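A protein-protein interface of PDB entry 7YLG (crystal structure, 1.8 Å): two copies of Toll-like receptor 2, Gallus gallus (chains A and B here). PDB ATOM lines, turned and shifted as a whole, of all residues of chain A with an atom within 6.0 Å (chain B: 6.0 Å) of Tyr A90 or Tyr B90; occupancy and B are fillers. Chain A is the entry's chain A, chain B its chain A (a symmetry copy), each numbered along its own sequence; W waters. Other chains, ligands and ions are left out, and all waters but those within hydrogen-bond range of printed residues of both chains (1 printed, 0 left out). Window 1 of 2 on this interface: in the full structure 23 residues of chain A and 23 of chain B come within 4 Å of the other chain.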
ATOM      1  N   ILE A  61     -11.929  15.491  -0.049  1.00  0.00           N
ATOM      2  CA  ILE A  61     -13.330  15.878   0.076  1.00  0.00           C
ATOM      3  C   ILE A  61     -13.504  17.305   0.553  1.00  0.00           C
ATOM      4  O   ILE A  61     -14.624  17.822   0.516  1.00  0.00           O
ATOM      5  CB  ILE A  61     -14.086  14.951   1.046  1.00  0.00           C
ATOM      6  CG1 ILE A  61     -13.379  14.931   2.402  1.00  0.00           C
ATOM      7  CG2 ILE A  61     -14.193  13.529   0.475  1.00  0.00           C
ATOM      8  CD1 ILE A  61     -14.205  14.239   3.520  1.00  0.00           C
ATOM      9  N   PHE A  62     -12.440  17.958   1.016  1.00  0.00           N
ATOM     10  CA  PHE A  62     -12.616  19.329   1.475  1.00  0.00           C
ATOM     11  C   PHE A  62     -12.636  20.324   0.320  1.00  0.00           C
ATOM     12  O   PHE A  62     -13.197  21.414   0.473  1.00  0.00           O
ATOM     13  CB  PHE A  62     -11.516  19.691   2.466  1.00  0.00           C
ATOM     14  CG  PHE A  62     -11.506  18.807   3.685  1.00  0.00           C
ATOM     15  CD1 PHE A  62     -12.274  19.124   4.780  1.00  0.00           C
ATOM     16  CD2 PHE A  62     -10.742  17.648   3.713  1.00  0.00           C
ATOM     17  CE1 PHE A  62     -12.274  18.294   5.919  1.00  0.00           C
ATOM     18  CE2 PHE A  62     -10.740  16.813   4.824  1.00  0.00           C
ATOM     19  CZ  PHE A  62     -11.500  17.142   5.927  1.00  0.00           C
ATOM     20  N   CYS A  85     -24.108   8.053   1.108  1.00  0.00           N
ATOM     21  CA  CYS A  85     -24.783   9.351   1.151  1.00  0.00           C
ATOM     22  C   CYS A  85     -24.913   9.854   2.582  1.00  0.00           C
ATOM     23  O   CYS A  85     -24.767  11.051   2.851  1.00  0.00           O
ATOM     24  CB  CYS A  85     -26.152   9.256   0.502  1.00  0.00           C
ATOM     25  SG  CYS A  85     -26.121   8.764  -1.203  1.00  0.00           S
ATOM     26  N   GLN A  86     -25.184   8.945   3.526  1.00  0.00           N
ATOM     27  CA  GLN A  86     -25.232   9.352   4.930  1.00  0.00           C
ATOM     28  C   GLN A  86     -23.901   9.907   5.403  1.00  0.00           C
ATOM     29  O   GLN A  86     -23.873  10.839   6.209  1.00  0.00           O
ATOM     30  CB  GLN A  86     -25.661   8.173   5.812  1.00  0.00           C
ATOM     31  CG  GLN A  86     -27.142   7.883   5.658  1.00  0.00           C
ATOM     32  CD  GLN A  86     -27.602   6.801   6.620  1.00  0.00           C
ATOM     33  OE1 GLN A  86     -26.934   6.542   7.610  1.00  0.00           O
ATOM     34  NE2 GLN A  86     -28.739   6.166   6.321  1.00  0.00           N
ATOM     35  N   TYR A  87     -22.789   9.314   4.974  1.00  0.00           N
ATOM     36  CA  TYR A  87     -21.497   9.872   5.357  1.00  0.00           C
ATOM     37  C   TYR A  87     -21.328  11.270   4.791  1.00  0.00           C
ATOM     38  O   TYR A  87     -20.734  12.142   5.435  1.00  0.00           O
ATOM     39  CB  TYR A  87     -20.366   9.007   4.841  1.00  0.00           C
ATOM     40  CG  TYR A  87     -20.074   7.834   5.730  1.00  0.00           C
ATOM     41  CD1 TYR A  87     -19.812   8.012   7.073  1.00  0.00           C
ATOM     42  CD2 TYR A  87     -20.057   6.549   5.214  1.00  0.00           C
ATOM     43  CE1 TYR A  87     -19.527   6.906   7.896  1.00  0.00           C
ATOM     44  CE2 TYR A  87     -19.786   5.465   6.021  1.00  0.00           C
ATOM     45  CZ  TYR A  87     -19.531   5.652   7.357  1.00  0.00           C
ATOM     46  OH  TYR A  87     -19.242   4.550   8.160  1.00  0.00           O
ATOM     47  N   GLU A  88     -21.801  11.471   3.565  1.00  0.00           N
ATOM     48  CA  GLU A  88     -21.697  12.784   2.919  1.00  0.00           C
ATOM     49  C   GLU A  88     -22.595  13.797   3.622  1.00  0.00           C
ATOM     50  O   GLU A  88     -22.194  14.947   3.861  1.00  0.00           O
ATOM     51  CB  GLU A  88     -22.046  12.642   1.423  1.00  0.00           C
ATOM     52  CG  GLU A  88     -21.738  13.884   0.567  1.00  0.00           C
ATOM     53  CD  GLU A  88     -21.548  13.557  -0.913  1.00  0.00           C
ATOM     54  OE1 GLU A  88     -22.419  12.890  -1.500  1.00  0.00           O
ATOM     55  OE2 GLU A  88     -20.510  13.948  -1.487  1.00  0.00           O
ATOM     56  N   LEU A  89     -23.796  13.369   4.008  1.00  0.00           N
ATOM     57  CA  LEU A  89     -24.669  14.215   4.822  1.00  0.00           C
ATOM     58  C   LEU A  89     -23.987  14.621   6.116  1.00  0.00           C
ATOM     59  O   LEU A  89     -23.971  15.805   6.474  1.00  0.00           O
ATOM     60  CB  LEU A  89     -25.974  13.486   5.141  1.00  0.00           C
ATOM     61  CG  LEU A  89     -27.235  13.942   4.406  1.00  0.00           C
ATOM     62  CD1 LEU A  89     -28.412  13.180   4.977  1.00  0.00           C
ATOM     63  CD2 LEU A  89     -27.442  15.448   4.522  1.00  0.00           C
ATOM     64  N   TYR A  90     -23.433  13.640   6.841  1.00  0.00           N
ATOM     65  CA  TYR A  90     -22.735  13.920   8.091  1.00  0.00           C
ATOM     66  C   TYR A  90     -21.683  14.999   7.893  1.00  0.00           C
ATOM     67  O   TYR A  90     -21.570  15.933   8.698  1.00  0.00           O
ATOM     68  CB  TYR A  90     -22.077  12.640   8.637  1.00  0.00           C
ATOM     69  CG  TYR A  90     -21.397  12.870   9.963  1.00  0.00           C
ATOM     70  CD1 TYR A  90     -22.114  12.815  11.151  1.00  0.00           C
ATOM     71  CD2 TYR A  90     -20.046  13.173  10.028  1.00  0.00           C
ATOM     72  CE1 TYR A  90     -21.501  13.039  12.359  1.00  0.00           C
ATOM     73  CE2 TYR A  90     -19.428  13.425  11.221  1.00  0.00           C
ATOM     74  CZ  TYR A  90     -20.154  13.352  12.393  1.00  0.00           C
ATOM     75  OH  TYR A  90     -19.514  13.581  13.586  1.00  0.00           O
ATOM     76  N   PHE A  91     -20.926  14.894   6.806  1.00  0.00           N
ATOM     77  CA  PHE A  91     -19.803  15.794   6.570  1.00  0.00           C
ATOM     78  C   PHE A  91     -20.289  17.211   6.347  1.00  0.00           C
ATOM     79  O   PHE A  91     -19.747  18.164   6.925  1.00  0.00           O
ATOM     80  CB  PHE A  91     -19.001  15.273   5.376  1.00  0.00           C
ATOM     81  CG  PHE A  91     -17.907  16.196   4.896  1.00  0.00           C
ATOM     82  CD1 PHE A  91     -16.712  16.290   5.581  1.00  0.00           C
ATOM     83  CD2 PHE A  91     -18.059  16.917   3.712  1.00  0.00           C
ATOM     84  CE1 PHE A  91     -15.697  17.113   5.139  1.00  0.00           C
ATOM     85  CE2 PHE A  91     -17.038  17.730   3.257  1.00  0.00           C
ATOM     86  CZ  PHE A  91     -15.865  17.836   3.965  1.00  0.00           C
ATOM     87  N   ALA A  92     -21.343  17.361   5.554  1.00  0.00           N
ATOM     88  CA  ALA A  92     -21.865  18.697   5.285  1.00  0.00           C
ATOM     89  C   ALA A  92     -22.468  19.290   6.546  1.00  0.00           C
ATOM     90  O   ALA A  92     -22.170  20.431   6.909  1.00  0.00           O
ATOM     91  CB  ALA A  92     -22.897  18.633   4.166  1.00  0.00           C
ATOM     92  N   GLU A  93     -23.317  18.517   7.228  1.00  0.00           N
ATOM     93  CA  GLU A  93     -23.843  18.928   8.523  1.00  0.00           C
ATOM     94  C   GLU A  93     -22.740  19.470   9.421  1.00  0.00           C
ATOM     95  O   GLU A  93     -22.842  20.591   9.930  1.00  0.00           O
ATOM     96  CB  GLU A  93     -24.562  17.749   9.186  1.00  0.00           C
ATOM     97  CG  GLU A  93     -24.943  17.934  10.660  1.00  0.00           C
ATOM     98  CD  GLU A  93     -26.351  17.415  11.006  1.00  0.00           C
ATOM     99  OE1 GLU A  93     -26.739  17.477  12.196  1.00  0.00           O
ATOM    100  OE2 GLU A  93     -27.077  16.971  10.092  1.00  0.00           O
ATOM    101  N   HIS A  94     -21.649  18.717   9.576  1.00  0.00           N
ATOM    102  CA  HIS A  94     -20.623  19.110  10.531  1.00  0.00           C
ATOM    103  C   HIS A  94     -19.645  20.142   9.994  1.00  0.00           C
ATOM    104  O   HIS A  94     -19.151  20.959  10.772  1.00  0.00           O
ATOM    105  CB  HIS A  94     -19.896  17.860  11.039  1.00  0.00           C
ATOM    106  CG  HIS A  94     -20.702  17.107  12.045  1.00  0.00           C
ATOM    107  ND1 HIS A  94     -21.889  16.484  11.724  1.00  0.00           N
ATOM    108  CD2 HIS A  94     -20.542  16.950  13.380  1.00  0.00           C
ATOM    109  CE1 HIS A  94     -22.414  15.953  12.813  1.00  0.00           C
ATOM    110  NE2 HIS A  94     -21.612  16.213  13.830  1.00  0.00           N
ATOM    111  N   ARG A  95     -19.358  20.154   8.694  1.00  0.00           N
ATOM    112  CA  ARG A  95     -18.567  21.243   8.131  1.00  0.00           C
ATOM    113  C   ARG A  95     -19.439  22.471   7.893  1.00  0.00           C
ATOM    114  O   ARG A  95     -19.123  23.570   8.356  1.00  0.00           O
ATOM    115  CB  ARG A  95     -17.898  20.810   6.821  1.00  0.00           C
ATOM    116  CG  ARG A  95     -16.739  19.858   6.982  1.00  0.00           C
ATOM    117  CD  ARG A  95     -15.518  20.548   7.572  1.00  0.00           C
ATOM    118  NE  ARG A  95     -14.987  21.584   6.690  1.00  0.00           N
ATOM    119  CZ  ARG A  95     -13.888  22.284   6.950  1.00  0.00           C
ATOM    120  NH1 ARG A  95     -13.208  22.053   8.065  1.00  0.00           N
ATOM    121  NH2 ARG A  95     -13.464  23.208   6.099  1.00  0.00           N
ATOM    122  N   PHE A 121     -29.116  12.973  12.448  1.00  0.00           N
ATOM    123  CA  PHE A 121     -28.956  14.072  11.484  1.00  0.00           C
ATOM    124  C   PHE A 121     -29.900  15.217  11.860  1.00  0.00           C
ATOM    125  O   PHE A 121     -30.823  15.565  11.129  1.00  0.00           O
ATOM    126  CB  PHE A 121     -29.223  13.593  10.061  1.00  0.00           C
ATOM    127  CG  PHE A 121     -28.189  12.640   9.527  1.00  0.00           C
ATOM    128  CD1 PHE A 121     -26.846  12.947   9.584  1.00  0.00           C
ATOM    129  CD2 PHE A 121     -28.565  11.423   8.987  1.00  0.00           C
ATOM    130  CE1 PHE A 121     -25.886  12.057   9.101  1.00  0.00           C
ATOM    131  CE2 PHE A 121     -27.614  10.532   8.504  1.00  0.00           C
ATOM    132  CZ  PHE A 121     -26.272  10.854   8.560  1.00  0.00           C
ATOM    133  N   ILE B  61     -25.525   4.940   9.609  1.00  0.00           N
ATOM    134  CA  ILE B  61     -24.088   4.832   9.839  1.00  0.00           C
ATOM    135  C   ILE B  61     -23.721   4.935  11.307  1.00  0.00           C
ATOM    136  O   ILE B  61     -22.570   4.666  11.659  1.00  0.00           O
ATOM    137  CB  ILE B  61     -23.312   5.920   9.073  1.00  0.00           C
ATOM    138  CG1 ILE B  61     -23.847   7.301   9.448  1.00  0.00           C
ATOM    139  CG2 ILE B  61     -23.412   5.698   7.555  1.00  0.00           C
ATOM    140  CD1 ILE B  61     -22.961   8.468   8.933  1.00  0.00           C
ATOM    141  N   PHE B  62     -24.652   5.327  12.171  1.00  0.00           N
ATOM    142  CA  PHE B  62     -24.290   5.426  13.579  1.00  0.00           C
ATOM    143  C   PHE B  62     -24.316   4.069  14.275  1.00  0.00           C
ATOM    144  O   PHE B  62     -23.638   3.902  15.294  1.00  0.00           O
ATOM    145  CB  PHE B  62     -25.221   6.402  14.289  1.00  0.00           C
ATOM    146  CG  PHE B  62     -25.167   7.793  13.714  1.00  0.00           C
ATOM    147  CD1 PHE B  62     -24.244   8.699  14.174  1.00  0.00           C
ATOM    148  CD2 PHE B  62     -26.030   8.170  12.693  1.00  0.00           C
ATOM    149  CE1 PHE B  62     -24.185   9.999  13.632  1.00  0.00           C
ATOM    150  CE2 PHE B  62     -25.977   9.444  12.140  1.00  0.00           C
ATOM    151  CZ  PHE B  62     -25.060  10.358  12.616  1.00  0.00           C
ATOM    152  N   CYS B  85     -14.068   6.669   1.198  1.00  0.00           N
ATOM    153  CA  CYS B  85     -13.271   6.334   2.379  1.00  0.00           C
ATOM    154  C   CYS B  85     -12.918   7.584   3.174  1.00  0.00           C
ATOM    155  O   CYS B  85     -12.916   7.571   4.410  1.00  0.00           O
ATOM    156  CB  CYS B  85     -12.007   5.598   1.972  1.00  0.00           C
ATOM    157  SG  CYS B  85     -12.294   4.072   1.112  1.00  0.00           S
ATOM    158  N   GLN B  86     -12.623   8.688   2.479  1.00  0.00           N
ATOM    159  CA  GLN B  86     -12.365   9.941   3.184  1.00  0.00           C
ATOM    160  C   GLN B  86     -13.569  10.393   3.991  1.00  0.00           C
ATOM    161  O   GLN B  86     -13.409  10.951   5.079  1.00  0.00           O
ATOM    162  CB  GLN B  86     -11.948  11.035   2.195  1.00  0.00           C
ATOM    163  CG  GLN B  86     -10.531  10.813   1.699  1.00  0.00           C
ATOM    164  CD  GLN B  86     -10.064  11.958   0.816  1.00  0.00           C
ATOM    165  OE1 GLN B  86     -10.626  13.041   0.872  1.00  0.00           O
ATOM    166  NE2 GLN B  86      -9.038  11.712  -0.004  1.00  0.00           N
ATOM    167  N   TYR B  87     -14.777  10.228   3.456  1.00  0.00           N
ATOM    168  CA  TYR B  87     -15.953  10.588   4.240  1.00  0.00           C
ATOM    169  C   TYR B  87     -16.055   9.722   5.484  1.00  0.00           C
ATOM    170  O   TYR B  87     -16.479  10.193   6.545  1.00  0.00           O
ATOM    171  CB  TYR B  87     -17.217  10.406   3.426  1.00  0.00           C
ATOM    172  CG  TYR B  87     -17.509  11.575   2.531  1.00  0.00           C
ATOM    173  CD1 TYR B  87     -17.586  12.854   3.040  1.00  0.00           C
ATOM    174  CD2 TYR B  87     -17.712  11.385   1.175  1.00  0.00           C
ATOM    175  CE1 TYR B  87     -17.874  13.942   2.195  1.00  0.00           C
ATOM    176  CE2 TYR B  87     -17.986  12.451   0.343  1.00  0.00           C
ATOM    177  CZ  TYR B  87     -18.057  13.722   0.860  1.00  0.00           C
ATOM    178  OH  TYR B  87     -18.349  14.789   0.013  1.00  0.00           O
ATOM    179  N   GLU B  88     -15.717   8.445   5.342  1.00  0.00           N
ATOM    180  CA  GLU B  88     -15.773   7.516   6.475  1.00  0.00           C
ATOM    181  C   GLU B  88     -14.702   7.865   7.503  1.00  0.00           C
ATOM    182  O   GLU B  88     -14.960   7.860   8.718  1.00  0.00           O
ATOM    183  CB  GLU B  88     -15.624   6.072   5.955  1.00  0.00           C
ATOM    184  CG  GLU B  88     -15.914   4.977   6.997  1.00  0.00           C
ATOM    185  CD  GLU B  88     -16.314   3.643   6.368  1.00  0.00           C
ATOM    186  OE1 GLU B  88     -15.590   3.152   5.484  1.00  0.00           O
ATOM    187  OE2 GLU B  88     -17.372   3.094   6.742  1.00  0.00           O
ATOM    188  N   LEU B  89     -13.510   8.227   7.032  1.00  0.00           N
ATOM    189  CA  LEU B  89     -12.468   8.725   7.927  1.00  0.00           C
ATOM    190  C   LEU B  89     -12.944   9.944   8.697  1.00  0.00           C
ATOM    191  O   LEU B  89     -12.801  10.008   9.924  1.00  0.00           O
ATOM    192  CB  LEU B  89     -11.209   9.083   7.137  1.00  0.00           C
ATOM    193  CG  LEU B  89     -10.009   8.143   7.255  1.00  0.00           C
ATOM    194  CD1 LEU B  89      -8.850   8.764   6.505  1.00  0.00           C
ATOM    195  CD2 LEU B  89      -9.646   7.874   8.711  1.00  0.00           C
ATOM    196  N   TYR B  90     -13.496  10.933   7.982  1.00  0.00           N
ATOM    197  CA  TYR B  90     -14.006  12.141   8.622  1.00  0.00           C
ATOM    198  C   TYR B  90     -14.965  11.792   9.749  1.00  0.00           C
ATOM    199  O   TYR B  90     -14.890  12.356  10.847  1.00  0.00           O
ATOM    200  CB  TYR B  90     -14.714  13.038   7.591  1.00  0.00           C
ATOM    201  CG  TYR B  90     -15.201  14.329   8.197  1.00  0.00           C
ATOM    202  CD1 TYR B  90     -14.351  15.421   8.327  1.00  0.00           C
ATOM    203  CD2 TYR B  90     -16.497  14.449   8.669  1.00  0.00           C
ATOM    204  CE1 TYR B  90     -14.789  16.594   8.894  1.00  0.00           C
ATOM    205  CE2 TYR B  90     -16.939  15.601   9.260  1.00  0.00           C
ATOM    206  CZ  TYR B  90     -16.086  16.682   9.369  1.00  0.00           C
ATOM    207  OH  TYR B  90     -16.549  17.840   9.939  1.00  0.00           O
ATOM    208  N   PHE B  91     -15.856  10.840   9.492  1.00  0.00           N
ATOM    209  CA  PHE B  91     -16.908  10.504  10.446  1.00  0.00           C
ATOM    210  C   PHE B  91     -16.319   9.903  11.704  1.00  0.00           C
ATOM    211  O   PHE B  91     -16.692  10.284  12.822  1.00  0.00           O
ATOM    212  CB  PHE B  91     -17.897   9.552   9.768  1.00  0.00           C
ATOM    213  CG  PHE B  91     -18.946   8.973  10.684  1.00  0.00           C
ATOM    214  CD1 PHE B  91     -20.035   9.727  11.077  1.00  0.00           C
ATOM    215  CD2 PHE B  91     -18.873   7.642  11.093  1.00  0.00           C
ATOM    216  CE1 PHE B  91     -21.013   9.200  11.896  1.00  0.00           C
ATOM    217  CE2 PHE B  91     -19.859   7.105  11.899  1.00  0.00           C
ATOM    218  CZ  PHE B  91     -20.920   7.876  12.306  1.00  0.00           C
ATOM    219  N   ALA B  92     -15.360   8.999  11.540  1.00  0.00           N
ATOM    220  CA  ALA B  92     -14.751   8.368  12.705  1.00  0.00           C
ATOM    221  C   ALA B  92     -13.942   9.386  13.491  1.00  0.00           C
ATOM    222  O   ALA B  92     -14.083   9.493  14.714  1.00  0.00           O
ATOM    223  CB  ALA B  92     -13.873   7.203  12.262  1.00  0.00           C
ATOM    224  N   GLU B  93     -13.095  10.148  12.796  1.00  0.00           N
ATOM    225  CA  GLU B  93     -12.377  11.251  13.424  1.00  0.00           C
ATOM    226  C   GLU B  93     -13.305  12.094  14.286  1.00  0.00           C
ATOM    227  O   GLU B  93     -13.034  12.308  15.473  1.00  0.00           O
ATOM    228  CB  GLU B  93     -11.699  12.105  12.347  1.00  0.00           C
ATOM    229  CG  GLU B  93     -11.125  13.448  12.816  1.00  0.00           C
ATOM    230  CD  GLU B  93      -9.742  13.771  12.220  1.00  0.00           C
ATOM    231  OE1 GLU B  93      -9.208  14.869  12.504  1.00  0.00           O
ATOM    232  OE2 GLU B  93      -9.179  12.924  11.494  1.00  0.00           O
ATOM    233  N   HIS B  94     -14.437  12.529  13.727  1.00  0.00           N
ATOM    234  CA  HIS B  94     -15.295  13.456  14.450  1.00  0.00           C
ATOM    235  C   HIS B  94     -16.227  12.785  15.444  1.00  0.00           C
ATOM    236  O   HIS B  94     -16.542  13.387  16.471  1.00  0.00           O
ATOM    237  CB  HIS B  94     -16.070  14.317  13.447  1.00  0.00           C
ATOM    238  CG  HIS B  94     -15.225  15.392  12.850  1.00  0.00           C
ATOM    239  ND1 HIS B  94     -14.151  15.117  12.029  1.00  0.00           N
ATOM    240  CD2 HIS B  94     -15.235  16.734  13.021  1.00  0.00           C
ATOM    241  CE1 HIS B  94     -13.551  16.246  11.700  1.00  0.00           C
ATOM    242  NE2 HIS B  94     -14.195  17.243  12.281  1.00  0.00           N
ATOM    243  N   ARG B  95     -16.669  11.553  15.194  1.00  0.00           N
ATOM    244  CA  ARG B  95     -17.414  10.825  16.215  1.00  0.00           C
ATOM    245  C   ARG B  95     -16.464  10.216  17.241  1.00  0.00           C
ATOM    246  O   ARG B  95     -16.615  10.430  18.447  1.00  0.00           O
ATOM    247  CB  ARG B  95     -18.277   9.728  15.581  1.00  0.00           C
ATOM    248  CG  ARG B  95     -19.493  10.223  14.839  1.00  0.00           C
ATOM    249  CD  ARG B  95     -20.561  10.744  15.789  1.00  0.00           C
ATOM    250  NE  ARG B  95     -21.094   9.694  16.654  1.00  0.00           N
ATOM    251  CZ  ARG B  95     -22.081   9.884  17.524  1.00  0.00           C
ATOM    252  NH1 ARG B  95     -22.637  11.082  17.638  1.00  0.00           N
ATOM    253  NH2 ARG B  95     -22.515   8.882  18.276  1.00  0.00           N
ATOM    254  N   PHE B 121      -7.262  15.963   7.919  1.00  0.00           N
ATOM    255  CA  PHE B 121      -7.432  14.783   8.780  1.00  0.00           C
ATOM    256  C   PHE B 121      -6.343  14.782   9.858  1.00  0.00           C
ATOM    257  O   PHE B 121      -5.488  13.903   9.915  1.00  0.00           O
ATOM    258  CB  PHE B 121      -7.388  13.498   7.962  1.00  0.00           C
ATOM    259  CG  PHE B 121      -8.567  13.310   7.046  1.00  0.00           C
ATOM    260  CD1 PHE B 121      -9.856  13.420   7.520  1.00  0.00           C
ATOM    261  CD2 PHE B 121      -8.378  13.044   5.702  1.00  0.00           C
ATOM    262  CE1 PHE B 121     -10.949  13.260   6.668  1.00  0.00           C
ATOM    263  CE2 PHE B 121      -9.462  12.883   4.847  1.00  0.00           C
ATOM    264  CZ  PHE B 121     -10.750  12.989   5.335  1.00  0.00           C
HETATM  265  O   HOH W   1     -18.494  12.060   7.124  1.00  0.00           O
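Of the printed residues of chain B, Ile A61 touches Gln B86 (2.9 Å) and Tyr B87 (3.7 Å). Tyr A90 touches four residues of chain B. Cys B85 touches none of the printed residues of chain A. Of chain A, only Tyr A90 (3.8 Å), Phe A91 (3.6 Å), His A94 (3.5 Å) and Arg A95 (3.6 Å) come within 4 Å of Tyr B90. Printed residues of chain A within 4 Å of Phe B91: Tyr A87 (3.3 Å) and Tyr A90 (3.6 Å). Glu B93 touches none of the printed residues of chain A. Printed residues of chain A within 4 Å of Phe B121: Phe A62. The nearest residue of chain B that does not touch Tyr A90 is Phe B62 (4.1 Å). The nearest printed residue of chain A that does not touch His B94 is His A94 (5.2 Å).
Tyr B87 touches its own counterpart, Tyr A87. Tyr A87 touches Phe B91, and with the chains exchanged Phe A91 touches Tyr B87. Tyr A90 touches Phe B91, and with the chains exchanged Phe A91 touches Tyr B90. Tyr A90 touches Arg B95, and with the chains exchanged Arg A95 touches Tyr B90. Positions printed for both chains: 61, 62, 85, 86, 87, 88, 89, 90, 91, 92, 93, 94, 95 and 121. Of the 18 pairs that touch across the chains among the printed residues, 18 have their exchanged pair printed and touching as well.
N of Ile A61 sits at hydrogen-bond distance from OE1 of Gln B86, 2.9 Å away. The backbone NH of Ile B61 is in hydrogen-bond range of the side-chain amide oxygen of Gln A86 (2.9 Å). The side-chain hydroxyl (OH) of Tyr A87 is in hydrogen-bond range of the side-chain carboxylate (OE2) of Glu B88 (2.8 Å). OE2 of Glu A88 sits at hydrogen-bond distance from OH of Tyr B87.
CD1 of Ile A61 touches CD1 of Tyr B87, 3.7 Å away. Phe A62 touches Phe B121. CD1 of Tyr A87 touches CD1 of Ile B61 (3.7 Å). Tyr B87 touches Tyr A87. Tyr A87 touches Phe B91. CE2 of Tyr A90 touches CE2 of Tyr B90, 3.8 Å away. Phe B91 touches Tyr A90. OH of Tyr A90 touches CB of His B94 (3.5 Å). His A94 touches Tyr B90 (CB to OH, 3.5 Å). Phe A121 touches Phe B62.
O of Tyr A90 lies within hydrogen-bond range of ND1 of His A94 (3.1 Å). The backbone carbonyl oxygen of Tyr B90 is in hydrogen-bond range of a ring nitrogen (ND1) of His B94 (3.1 Å).
Water W1 lies within hydrogen-bond range of O of Tyr A87 (2.8 Å) and O of Tyr B87 (2.8 Å).
Of the 14 printed residues of chain B, 10 touch a printed residue of chain A. Hydrophobic or aromatic side chains of chain B within 4 Å of the printed part of chain A: Ile B61, Phe B62, Tyr B87, Tyr B90, Phe B91, His B94 and Phe B121. Of the 14 printed residues of chain A, 10 touch a printed residue of chain B. Among the printed residues, no Asp or Glu carboxylate lies within 4 Å of a Lys or Arg side-chain nitrogen of the other chain.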
